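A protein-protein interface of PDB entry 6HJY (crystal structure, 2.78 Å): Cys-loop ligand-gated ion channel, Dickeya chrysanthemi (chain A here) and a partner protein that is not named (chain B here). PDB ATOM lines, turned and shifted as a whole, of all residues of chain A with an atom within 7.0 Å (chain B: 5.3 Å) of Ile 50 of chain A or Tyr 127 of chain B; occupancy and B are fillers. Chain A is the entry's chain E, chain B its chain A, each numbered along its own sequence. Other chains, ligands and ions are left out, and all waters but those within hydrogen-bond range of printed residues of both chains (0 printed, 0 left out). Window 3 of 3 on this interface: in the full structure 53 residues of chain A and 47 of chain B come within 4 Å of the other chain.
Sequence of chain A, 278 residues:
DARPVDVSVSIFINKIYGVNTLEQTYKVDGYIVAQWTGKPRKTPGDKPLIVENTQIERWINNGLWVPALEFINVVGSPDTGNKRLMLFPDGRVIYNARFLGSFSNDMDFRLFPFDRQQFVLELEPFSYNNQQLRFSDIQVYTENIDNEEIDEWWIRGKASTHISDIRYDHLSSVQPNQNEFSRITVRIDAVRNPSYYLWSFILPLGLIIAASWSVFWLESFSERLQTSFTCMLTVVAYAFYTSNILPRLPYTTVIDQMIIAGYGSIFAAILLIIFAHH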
ATOM      1  N   LYS A  47     -23.342  16.557  18.114  1.00  0.00           N
ATOM      2  CA  LYS A  47     -21.906  16.285  18.134  1.00  0.00           C
ATOM      3  C   LYS A  47     -21.213  17.651  17.979  1.00  0.00           C
ATOM      4  O   LYS A  47     -21.851  18.563  17.444  1.00  0.00           O
ATOM      5  CB  LYS A  47     -21.525  15.383  16.942  1.00  0.00           C
ATOM      6  CG  LYS A  47     -22.306  14.079  16.853  1.00  0.00           C
ATOM      7  CD  LYS A  47     -21.414  12.870  17.066  1.00  0.00           C
ATOM      8  CE  LYS A  47     -22.194  11.579  16.995  1.00  0.00           C
ATOM      9  NZ  LYS A  47     -22.999  11.350  18.227  1.00  0.00           N
ATOM     10  N   PRO A  48     -19.927  17.844  18.368  1.00  0.00           N
ATOM     11  CA  PRO A  48     -19.307  19.169  18.172  1.00  0.00           C
ATOM     12  C   PRO A  48     -19.329  19.641  16.719  1.00  0.00           C
ATOM     13  O   PRO A  48     -19.382  18.828  15.789  1.00  0.00           O
ATOM     14  CB  PRO A  48     -17.873  18.977  18.674  1.00  0.00           C
ATOM     15  CG  PRO A  48     -17.938  17.802  19.566  1.00  0.00           C
ATOM     16  CD  PRO A  48     -18.987  16.902  19.009  1.00  0.00           C
ATOM     17  N   LEU A  49     -19.331  20.967  16.537  1.00  0.00           N
ATOM     18  CA  LEU A  49     -19.366  21.591  15.218  1.00  0.00           C
ATOM     19  C   LEU A  49     -18.058  22.320  14.911  1.00  0.00           C
ATOM     20  O   LEU A  49     -17.583  23.116  15.726  1.00  0.00           O
ATOM     21  CB  LEU A  49     -20.599  22.514  15.104  1.00  0.00           C
ATOM     22  CG  LEU A  49     -20.771  23.391  13.850  1.00  0.00           C
ATOM     23  CD1 LEU A  49     -20.862  22.564  12.568  1.00  0.00           C
ATOM     24  CD2 LEU A  49     -21.995  24.250  13.982  1.00  0.00           C
ATOM     25  N   ILE A  50     -17.471  22.014  13.744  1.00  0.00           N
ATOM     26  CA  ILE A  50     -16.222  22.615  13.296  1.00  0.00           C
ATOM     27  C   ILE A  50     -16.515  23.712  12.274  1.00  0.00           C
ATOM     28  O   ILE A  50     -17.151  23.463  11.247  1.00  0.00           O
ATOM     29  CB  ILE A  50     -15.191  21.549  12.826  1.00  0.00           C
ATOM     30  CG1 ILE A  50     -14.489  20.926  14.046  1.00  0.00           C
ATOM     31  CG2 ILE A  50     -14.160  22.141  11.854  1.00  0.00           C
ATOM     32  CD1 ILE A  50     -14.078  19.485  13.847  1.00  0.00           C
ATOM     33  N   VAL A  51     -16.091  24.941  12.594  1.00  0.00           N
ATOM     34  CA  VAL A  51     -16.233  26.120  11.735  1.00  0.00           C
ATOM     35  C   VAL A  51     -14.814  26.644  11.540  1.00  0.00           C
ATOM     36  O   VAL A  51     -14.115  26.902  12.522  1.00  0.00           O
ATOM     37  CB  VAL A  51     -17.135  27.224  12.353  1.00  0.00           C
ATOM     38  CG1 VAL A  51     -17.463  28.291  11.330  1.00  0.00           C
ATOM     39  CG2 VAL A  51     -18.421  26.659  12.953  1.00  0.00           C
ATOM     40  N   GLU A  52     -14.363  26.762  10.297  1.00  0.00           N
ATOM     41  CA  GLU A  52     -13.003  27.238  10.118  1.00  0.00           C
ATOM     42  C   GLU A  52     -12.840  28.316   9.073  1.00  0.00           C
ATOM     43  O   GLU A  52     -13.651  28.447   8.146  1.00  0.00           O
ATOM     44  CB  GLU A  52     -12.028  26.061   9.863  1.00  0.00           C
ATOM     45  CG  GLU A  52     -12.271  25.263   8.585  1.00  0.00           C
ATOM     46  CD  GLU A  52     -11.407  24.036   8.380  1.00  0.00           C
ATOM     47  OE1 GLU A  52     -10.428  23.851   9.132  1.00  0.00           O
ATOM     48  OE2 GLU A  52     -11.706  23.262   7.446  1.00  0.00           O
ATOM     49  N   GLN A  55     -15.475  31.218   7.543  1.00  0.00           N
ATOM     50  CA  GLN A  55     -16.805  30.909   8.082  1.00  0.00           C
ATOM     51  C   GLN A  55     -16.988  31.403   9.516  1.00  0.00           C
ATOM     52  O   GLN A  55     -18.128  31.632   9.921  1.00  0.00           O
ATOM     53  CB  GLN A  55     -17.129  29.414   7.964  1.00  0.00           C
ATOM     54  CG  GLN A  55     -17.134  28.880   6.523  1.00  0.00           C
ATOM     55  CD  GLN A  55     -17.964  29.695   5.563  1.00  0.00           C
ATOM     56  OE1 GLN A  55     -19.136  29.985   5.808  1.00  0.00           O
ATOM     57  NE2 GLN A  55     -17.384  30.002   4.423  1.00  0.00           N
ATOM     58  N   TRP A  59     -20.199  33.527  11.502  1.00  0.00           N
ATOM     59  CA  TRP A  59     -20.751  33.234  12.825  1.00  0.00           C
ATOM     60  C   TRP A  59     -20.710  34.451  13.730  1.00  0.00           C
ATOM     61  O   TRP A  59     -21.636  34.642  14.516  1.00  0.00           O
ATOM     62  CB  TRP A  59     -20.015  32.055  13.475  1.00  0.00           C
ATOM     63  CG  TRP A  59     -20.520  30.735  12.990  1.00  0.00           C
ATOM     64  CD1 TRP A  59     -20.270  30.156  11.781  1.00  0.00           C
ATOM     65  CD2 TRP A  59     -21.429  29.867  13.671  1.00  0.00           C
ATOM     66  NE1 TRP A  59     -20.945  28.963  11.676  1.00  0.00           N
ATOM     67  CE2 TRP A  59     -21.665  28.759  12.825  1.00  0.00           C
ATOM     68  CE3 TRP A  59     -22.055  29.907  14.927  1.00  0.00           C
ATOM     69  CZ2 TRP A  59     -22.512  27.707  13.189  1.00  0.00           C
ATOM     70  CZ3 TRP A  59     -22.897  28.867  15.285  1.00  0.00           C
ATOM     71  CH2 TRP A  59     -23.107  27.775  14.431  1.00  0.00           C
ATOM     72  N   ARG A  84      -9.838  27.788  13.475  1.00  0.00           N
ATOM     73  CA  ARG A  84     -11.057  27.060  13.538  1.00  0.00           C
ATOM     74  C   ARG A  84     -11.781  27.459  14.859  1.00  0.00           C
ATOM     75  O   ARG A  84     -11.279  28.230  15.691  1.00  0.00           O
ATOM     76  CB  ARG A  84     -10.752  25.566  13.425  1.00  0.00           C
ATOM     77  CG  ARG A  84     -10.416  24.947  14.753  1.00  0.00           C
ATOM     78  CD  ARG A  84     -10.534  23.468  14.863  1.00  0.00           C
ATOM     79  NE  ARG A  84      -9.795  22.973  16.033  1.00  0.00           N
ATOM     80  CZ  ARG A  84     -10.311  22.784  17.250  1.00  0.00           C
ATOM     81  NH1 ARG A  84     -11.583  23.058  17.491  1.00  0.00           N
ATOM     82  NH2 ARG A  84      -9.546  22.327  18.239  1.00  0.00           N
ATOM     83  N   LEU A  85     -13.003  26.917  15.037  1.00  0.00           N
ATOM     84  CA  LEU A  85     -13.902  27.001  16.190  1.00  0.00           C
ATOM     85  C   LEU A  85     -14.573  25.663  16.342  1.00  0.00           C
ATOM     86  O   LEU A  85     -15.066  25.097  15.357  1.00  0.00           O
ATOM     87  CB  LEU A  85     -14.971  28.099  16.053  1.00  0.00           C
ATOM     88  CG  LEU A  85     -14.541  29.492  16.471  1.00  0.00           C
ATOM     89  CD1 LEU A  85     -15.598  30.486  16.145  1.00  0.00           C
ATOM     90  CD2 LEU A  85     -14.215  29.580  17.945  1.00  0.00           C
ATOM     91  N   MET A  86     -14.506  25.116  17.553  1.00  0.00           N
ATOM     92  CA  MET A  86     -15.190  23.876  17.892  1.00  0.00           C
ATOM     93  C   MET A  86     -16.229  24.314  18.875  1.00  0.00           C
ATOM     94  O   MET A  86     -15.894  24.788  19.971  1.00  0.00           O
ATOM     95  CB  MET A  86     -14.280  22.817  18.514  1.00  0.00           C
ATOM     96  CG  MET A  86     -14.909  21.442  18.563  1.00  0.00           C
ATOM     97  SD  MET A  86     -13.735  20.129  18.944  1.00  0.00           S
ATOM     98  CE  MET A  86     -13.096  19.814  17.352  1.00  0.00           C
ATOM     99  N   LEU A  87     -17.485  24.257  18.432  1.00  0.00           N
ATOM    100  CA  LEU A  87     -18.638  24.635  19.228  1.00  0.00           C
ATOM    101  C   LEU A  87     -19.324  23.354  19.674  1.00  0.00           C
ATOM    102  O   LEU A  87     -19.733  22.535  18.844  1.00  0.00           O
ATOM    103  CB  LEU A  87     -19.600  25.533  18.430  1.00  0.00           C
ATOM    104  CG  LEU A  87     -18.997  26.701  17.649  1.00  0.00           C
ATOM    105  CD1 LEU A  87     -19.970  27.201  16.615  1.00  0.00           C
ATOM    106  CD2 LEU A  87     -18.559  27.833  18.574  1.00  0.00           C
ATOM    107  N   TRP B  64     -18.618  21.373   1.868  1.00  0.00           N
ATOM    108  CA  TRP B  64     -17.561  20.976   2.789  1.00  0.00           C
ATOM    109  C   TRP B  64     -16.218  20.905   2.068  1.00  0.00           C
ATOM    110  O   TRP B  64     -16.030  20.079   1.176  1.00  0.00           O
ATOM    111  CB  TRP B  64     -17.916  19.645   3.472  1.00  0.00           C
ATOM    112  CG  TRP B  64     -16.960  19.198   4.546  1.00  0.00           C
ATOM    113  CD1 TRP B  64     -16.852  19.700   5.809  1.00  0.00           C
ATOM    114  CD2 TRP B  64     -16.049  18.090   4.475  1.00  0.00           C
ATOM    115  NE1 TRP B  64     -15.904  18.997   6.523  1.00  0.00           N
ATOM    116  CE2 TRP B  64     -15.396  18.001   5.727  1.00  0.00           C
ATOM    117  CE3 TRP B  64     -15.703  17.175   3.466  1.00  0.00           C
ATOM    118  CZ2 TRP B  64     -14.416  17.037   5.996  1.00  0.00           C
ATOM    119  CZ3 TRP B  64     -14.742  16.210   3.736  1.00  0.00           C
ATOM    120  CH2 TRP B  64     -14.106  16.149   4.986  1.00  0.00           C
ATOM    121  N   PRO B  66     -12.499  20.804   3.558  1.00  0.00           N
ATOM    122  CA  PRO B  66     -11.647  20.819   4.761  1.00  0.00           C
ATOM    123  C   PRO B  66     -10.301  21.505   4.541  1.00  0.00           C
ATOM    124  O   PRO B  66      -9.725  21.404   3.454  1.00  0.00           O
ATOM    125  CB  PRO B  66     -11.474  19.339   5.084  1.00  0.00           C
ATOM    126  CG  PRO B  66     -11.620  18.645   3.757  1.00  0.00           C
ATOM    127  CD  PRO B  66     -12.637  19.442   2.998  1.00  0.00           C
ATOM    128  N   ALA B  67      -9.807  22.225   5.568  1.00  0.00           N
ATOM    129  CA  ALA B  67      -8.526  22.913   5.482  1.00  0.00           C
ATOM    130  C   ALA B  67      -7.406  21.951   5.804  1.00  0.00           C
ATOM    131  O   ALA B  67      -7.389  21.326   6.878  1.00  0.00           O
ATOM    132  CB  ALA B  67      -8.485  24.109   6.417  1.00  0.00           C
ATOM    133  N   PRO B 124      -4.836  17.493   8.073  1.00  0.00           N
ATOM    134  CA  PRO B 124      -6.071  18.292   8.191  1.00  0.00           C
ATOM    135  C   PRO B 124      -5.985  19.153   9.448  1.00  0.00           C
ATOM    136  O   PRO B 124      -5.469  18.695  10.472  1.00  0.00           O
ATOM    137  CB  PRO B 124      -7.177  17.235   8.314  1.00  0.00           C
ATOM    138  CG  PRO B 124      -6.577  15.993   7.821  1.00  0.00           C
ATOM    139  CD  PRO B 124      -5.136  16.055   8.184  1.00  0.00           C
ATOM    140  N   PHE B 125      -6.410  20.413   9.352  1.00  0.00           N
ATOM    141  CA  PHE B 125      -6.285  21.334  10.476  1.00  0.00           C
ATOM    142  C   PHE B 125      -7.234  21.044  11.644  1.00  0.00           C
ATOM    143  O   PHE B 125      -6.845  21.232  12.798  1.00  0.00           O
ATOM    144  CB  PHE B 125      -6.425  22.797   9.994  1.00  0.00           C
ATOM    145  CG  PHE B 125      -6.105  23.844  11.040  1.00  0.00           C
ATOM    146  CD1 PHE B 125      -4.786  24.150  11.363  1.00  0.00           C
ATOM    147  CD2 PHE B 125      -7.122  24.519  11.705  1.00  0.00           C
ATOM    148  CE1 PHE B 125      -4.491  25.112  12.340  1.00  0.00           C
ATOM    149  CE2 PHE B 125      -6.824  25.473  12.689  1.00  0.00           C
ATOM    150  CZ  PHE B 125      -5.512  25.767  12.990  1.00  0.00           C
ATOM    151  N   SER B 126      -8.459  20.595  11.357  1.00  0.00           N
ATOM    152  CA  SER B 126      -9.501  20.434  12.367  1.00  0.00           C
ATOM    153  C   SER B 126     -10.108  19.028  12.475  1.00  0.00           C
ATOM    154  O   SER B 126     -10.671  18.681  13.523  1.00  0.00           O
ATOM    155  CB  SER B 126     -10.623  21.425  12.068  1.00  0.00           C
ATOM    156  OG  SER B 126     -10.189  22.676  11.550  1.00  0.00           O
ATOM    157  N   TYR B 127     -10.033  18.243  11.389  1.00  0.00           N
ATOM    158  CA  TYR B 127     -10.621  16.909  11.337  1.00  0.00           C
ATOM    159  C   TYR B 127      -9.654  15.789  11.642  1.00  0.00           C
ATOM    160  O   TYR B 127      -8.666  15.591  10.923  1.00  0.00           O
ATOM    161  CB  TYR B 127     -11.319  16.682   9.988  1.00  0.00           C
ATOM    162  CG  TYR B 127     -12.396  17.712   9.722  1.00  0.00           C
ATOM    163  CD1 TYR B 127     -13.633  17.634  10.359  1.00  0.00           C
ATOM    164  CD2 TYR B 127     -12.170  18.783   8.865  1.00  0.00           C
ATOM    165  CE1 TYR B 127     -14.620  18.595  10.138  1.00  0.00           C
ATOM    166  CE2 TYR B 127     -13.153  19.742   8.629  1.00  0.00           C
ATOM    167  CZ  TYR B 127     -14.379  19.638   9.261  1.00  0.00           C
ATOM    168  OH  TYR B 127     -15.337  20.587   9.034  1.00  0.00           O
ATOM    169  N   ASN B 128      -9.966  15.030  12.712  1.00  0.00           N
ATOM    170  CA  ASN B 128      -9.206  13.856  13.137  1.00  0.00           C
ATOM    171  C   ASN B 128      -9.449  12.691  12.133  1.00  0.00           C
ATOM    172  O   ASN B 128     -10.354  12.795  11.302  1.00  0.00           O
ATOM    173  CB  ASN B 128      -9.536  13.484  14.597  1.00  0.00           C
ATOM    174  CG  ASN B 128     -10.923  12.934  14.834  1.00  0.00           C
ATOM    175  OD1 ASN B 128     -11.409  12.052  14.127  1.00  0.00           O
ATOM    176  ND2 ASN B 128     -11.584  13.419  15.864  1.00  0.00           N
ATOM    177  N   ASN B 129      -8.656  11.594  12.218  1.00  0.00           N
ATOM    178  CA  ASN B 129      -8.701  10.427  11.315  1.00  0.00           C
ATOM    179  C   ASN B 129     -10.008   9.589  11.362  1.00  0.00           C
ATOM    180  O   ASN B 129     -10.151   8.657  10.571  1.00  0.00           O
ATOM    181  CB  ASN B 129      -7.485   9.526  11.539  1.00  0.00           C
ATOM    182  CG  ASN B 129      -7.298   9.015  12.950  1.00  0.00           C
ATOM    183  OD1 ASN B 129      -8.229   8.932  13.770  1.00  0.00           O
ATOM    184  ND2 ASN B 129      -6.080   8.610  13.242  1.00  0.00           N
ATOM    185  N   GLN B 131     -12.851  11.207  11.156  1.00  0.00           N
ATOM    186  CA  GLN B 131     -13.610  12.115  10.298  1.00  0.00           C
ATOM    187  C   GLN B 131     -12.957  12.235   8.925  1.00  0.00           C
ATOM    188  O   GLN B 131     -13.659  12.217   7.915  1.00  0.00           O
ATOM    189  CB  GLN B 131     -13.701  13.516  10.945  1.00  0.00           C
ATOM    190  CG  GLN B 131     -14.322  13.533  12.336  1.00  0.00           C
ATOM    191  CD  GLN B 131     -14.271  14.907  12.929  1.00  0.00           C
ATOM    192  OE1 GLN B 131     -13.261  15.334  13.496  1.00  0.00           O
ATOM    193  NE2 GLN B 131     -15.365  15.635  12.810  1.00  0.00           N
ATOM    194  N   LEU B 132     -11.621  12.366   8.889  1.00  0.00           N
ATOM    195  CA  LEU B 132     -10.855  12.543   7.658  1.00  0.00           C
ATOM    196  C   LEU B 132      -9.500  11.852   7.715  1.00  0.00           C
ATOM    197  O   LEU B 132      -8.647  12.207   8.535  1.00  0.00           O
ATOM    198  CB  LEU B 132     -10.657  14.053   7.412  1.00  0.00           C
ATOM    199  CG  LEU B 132     -10.330  14.534   6.002  1.00  0.00           C
ATOM    200  CD1 LEU B 132     -10.472  16.010   5.934  1.00  0.00           C
ATOM    201  CD2 LEU B 132      -8.891  14.217   5.616  1.00  0.00           C
ATOM    202  N   PHE B 180      -4.557  12.309  14.217  1.00  0.00           N
ATOM    203  CA  PHE B 180      -4.666  13.002  12.929  1.00  0.00           C
ATOM    204  C   PHE B 180      -3.849  12.318  11.834  1.00  0.00           C
ATOM    205  O   PHE B 180      -2.720  11.887  12.070  1.00  0.00           O
ATOM    206  CB  PHE B 180      -4.261  14.481  13.065  1.00  0.00           C
ATOM    207  CG  PHE B 180      -5.320  15.376  13.674  1.00  0.00           C
ATOM    208  CD1 PHE B 180      -5.527  15.403  15.051  1.00  0.00           C
ATOM    209  CD2 PHE B 180      -6.096  16.204  12.873  1.00  0.00           C
ATOM    210  CE1 PHE B 180      -6.513  16.220  15.611  1.00  0.00           C
ATOM    211  CE2 PHE B 180      -7.069  17.037  13.440  1.00  0.00           C
ATOM    212  CZ  PHE B 180      -7.272  17.033  14.803  1.00  0.00           C
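The side-chain hydroxyl (OH) of Tyr 127 of chain B lies within hydrogen-bond range of the indole nitrogen (NE1) of Trp 64 of chain B (3.0 Å).
N of Phe 125 of chain B lies within hydrogen-bond range of O of Ala 67 of chain B.
OG of Ser 126 of chain B sits at hydrogen-bond distance from OE1 of Glu 52 of chain A.
The backbone NH (N) of Ala 67 of chain B lies within hydrogen-bond range of the side-chain carboxylate (OE2) of Glu 52 of chain A (2.9 Å).
Among the printed residues, merely in contact across the chains: Ile 50 of chain A with Ser 126 of chain B (3.5 Å), Ile 50 of chain A with Tyr 127 of chain B (3.4 Å), Glu 52 of chain A with Pro 66 of chain B (3.6 Å), Glu 52 of chain A with Tyr 127 of chain B (3.99 Å), Arg 84 of chain A with Phe 125 of chain B (3.9 Å) and Arg 84 of chain A with Ser 126 of chain B (3.4 Å).
Printed residues of chain B that touch a printed residue of chain A: Pro 66, Ala 67, Phe 125, Ser 126 and Tyr 127.
Hydrophobic or aromatic side chains of chain B that line the printed part of chain A: Ala 67, Phe 125 and Tyr 127.
Hydrophobic or aromatic side chains of chain A that line the printed part of chain B: Ile 50.
Among the printed residues, no Asp or Glu carboxylate lies within 4 Å of a Lys or Arg side-chain nitrogen of the other chain.
Ile 50 of chain A touches just these residues of chain B: Ser 126 and Tyr 127.
Val 51 of chain A touches none of the printed residues of chain B.
Printed residues of chain B within 4 Å of Arg 84 of chain A: Phe 125 and Ser 126.
Of the printed residues of chain A, Pro 66 of chain B touches Glu 52.
Of the printed residues of chain A, Ala 67 of chain B touches Glu 52.
Of the printed residues of chain A, Ser 126 of chain B touches Ile 50 (3.5 Å), Glu 52 (2.7 Å) and Arg 84 (3.4 Å).
The nearest residue of chain B that does not touch Ile 50 of chain A is Gln 131 of chain B (4.2 Å).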
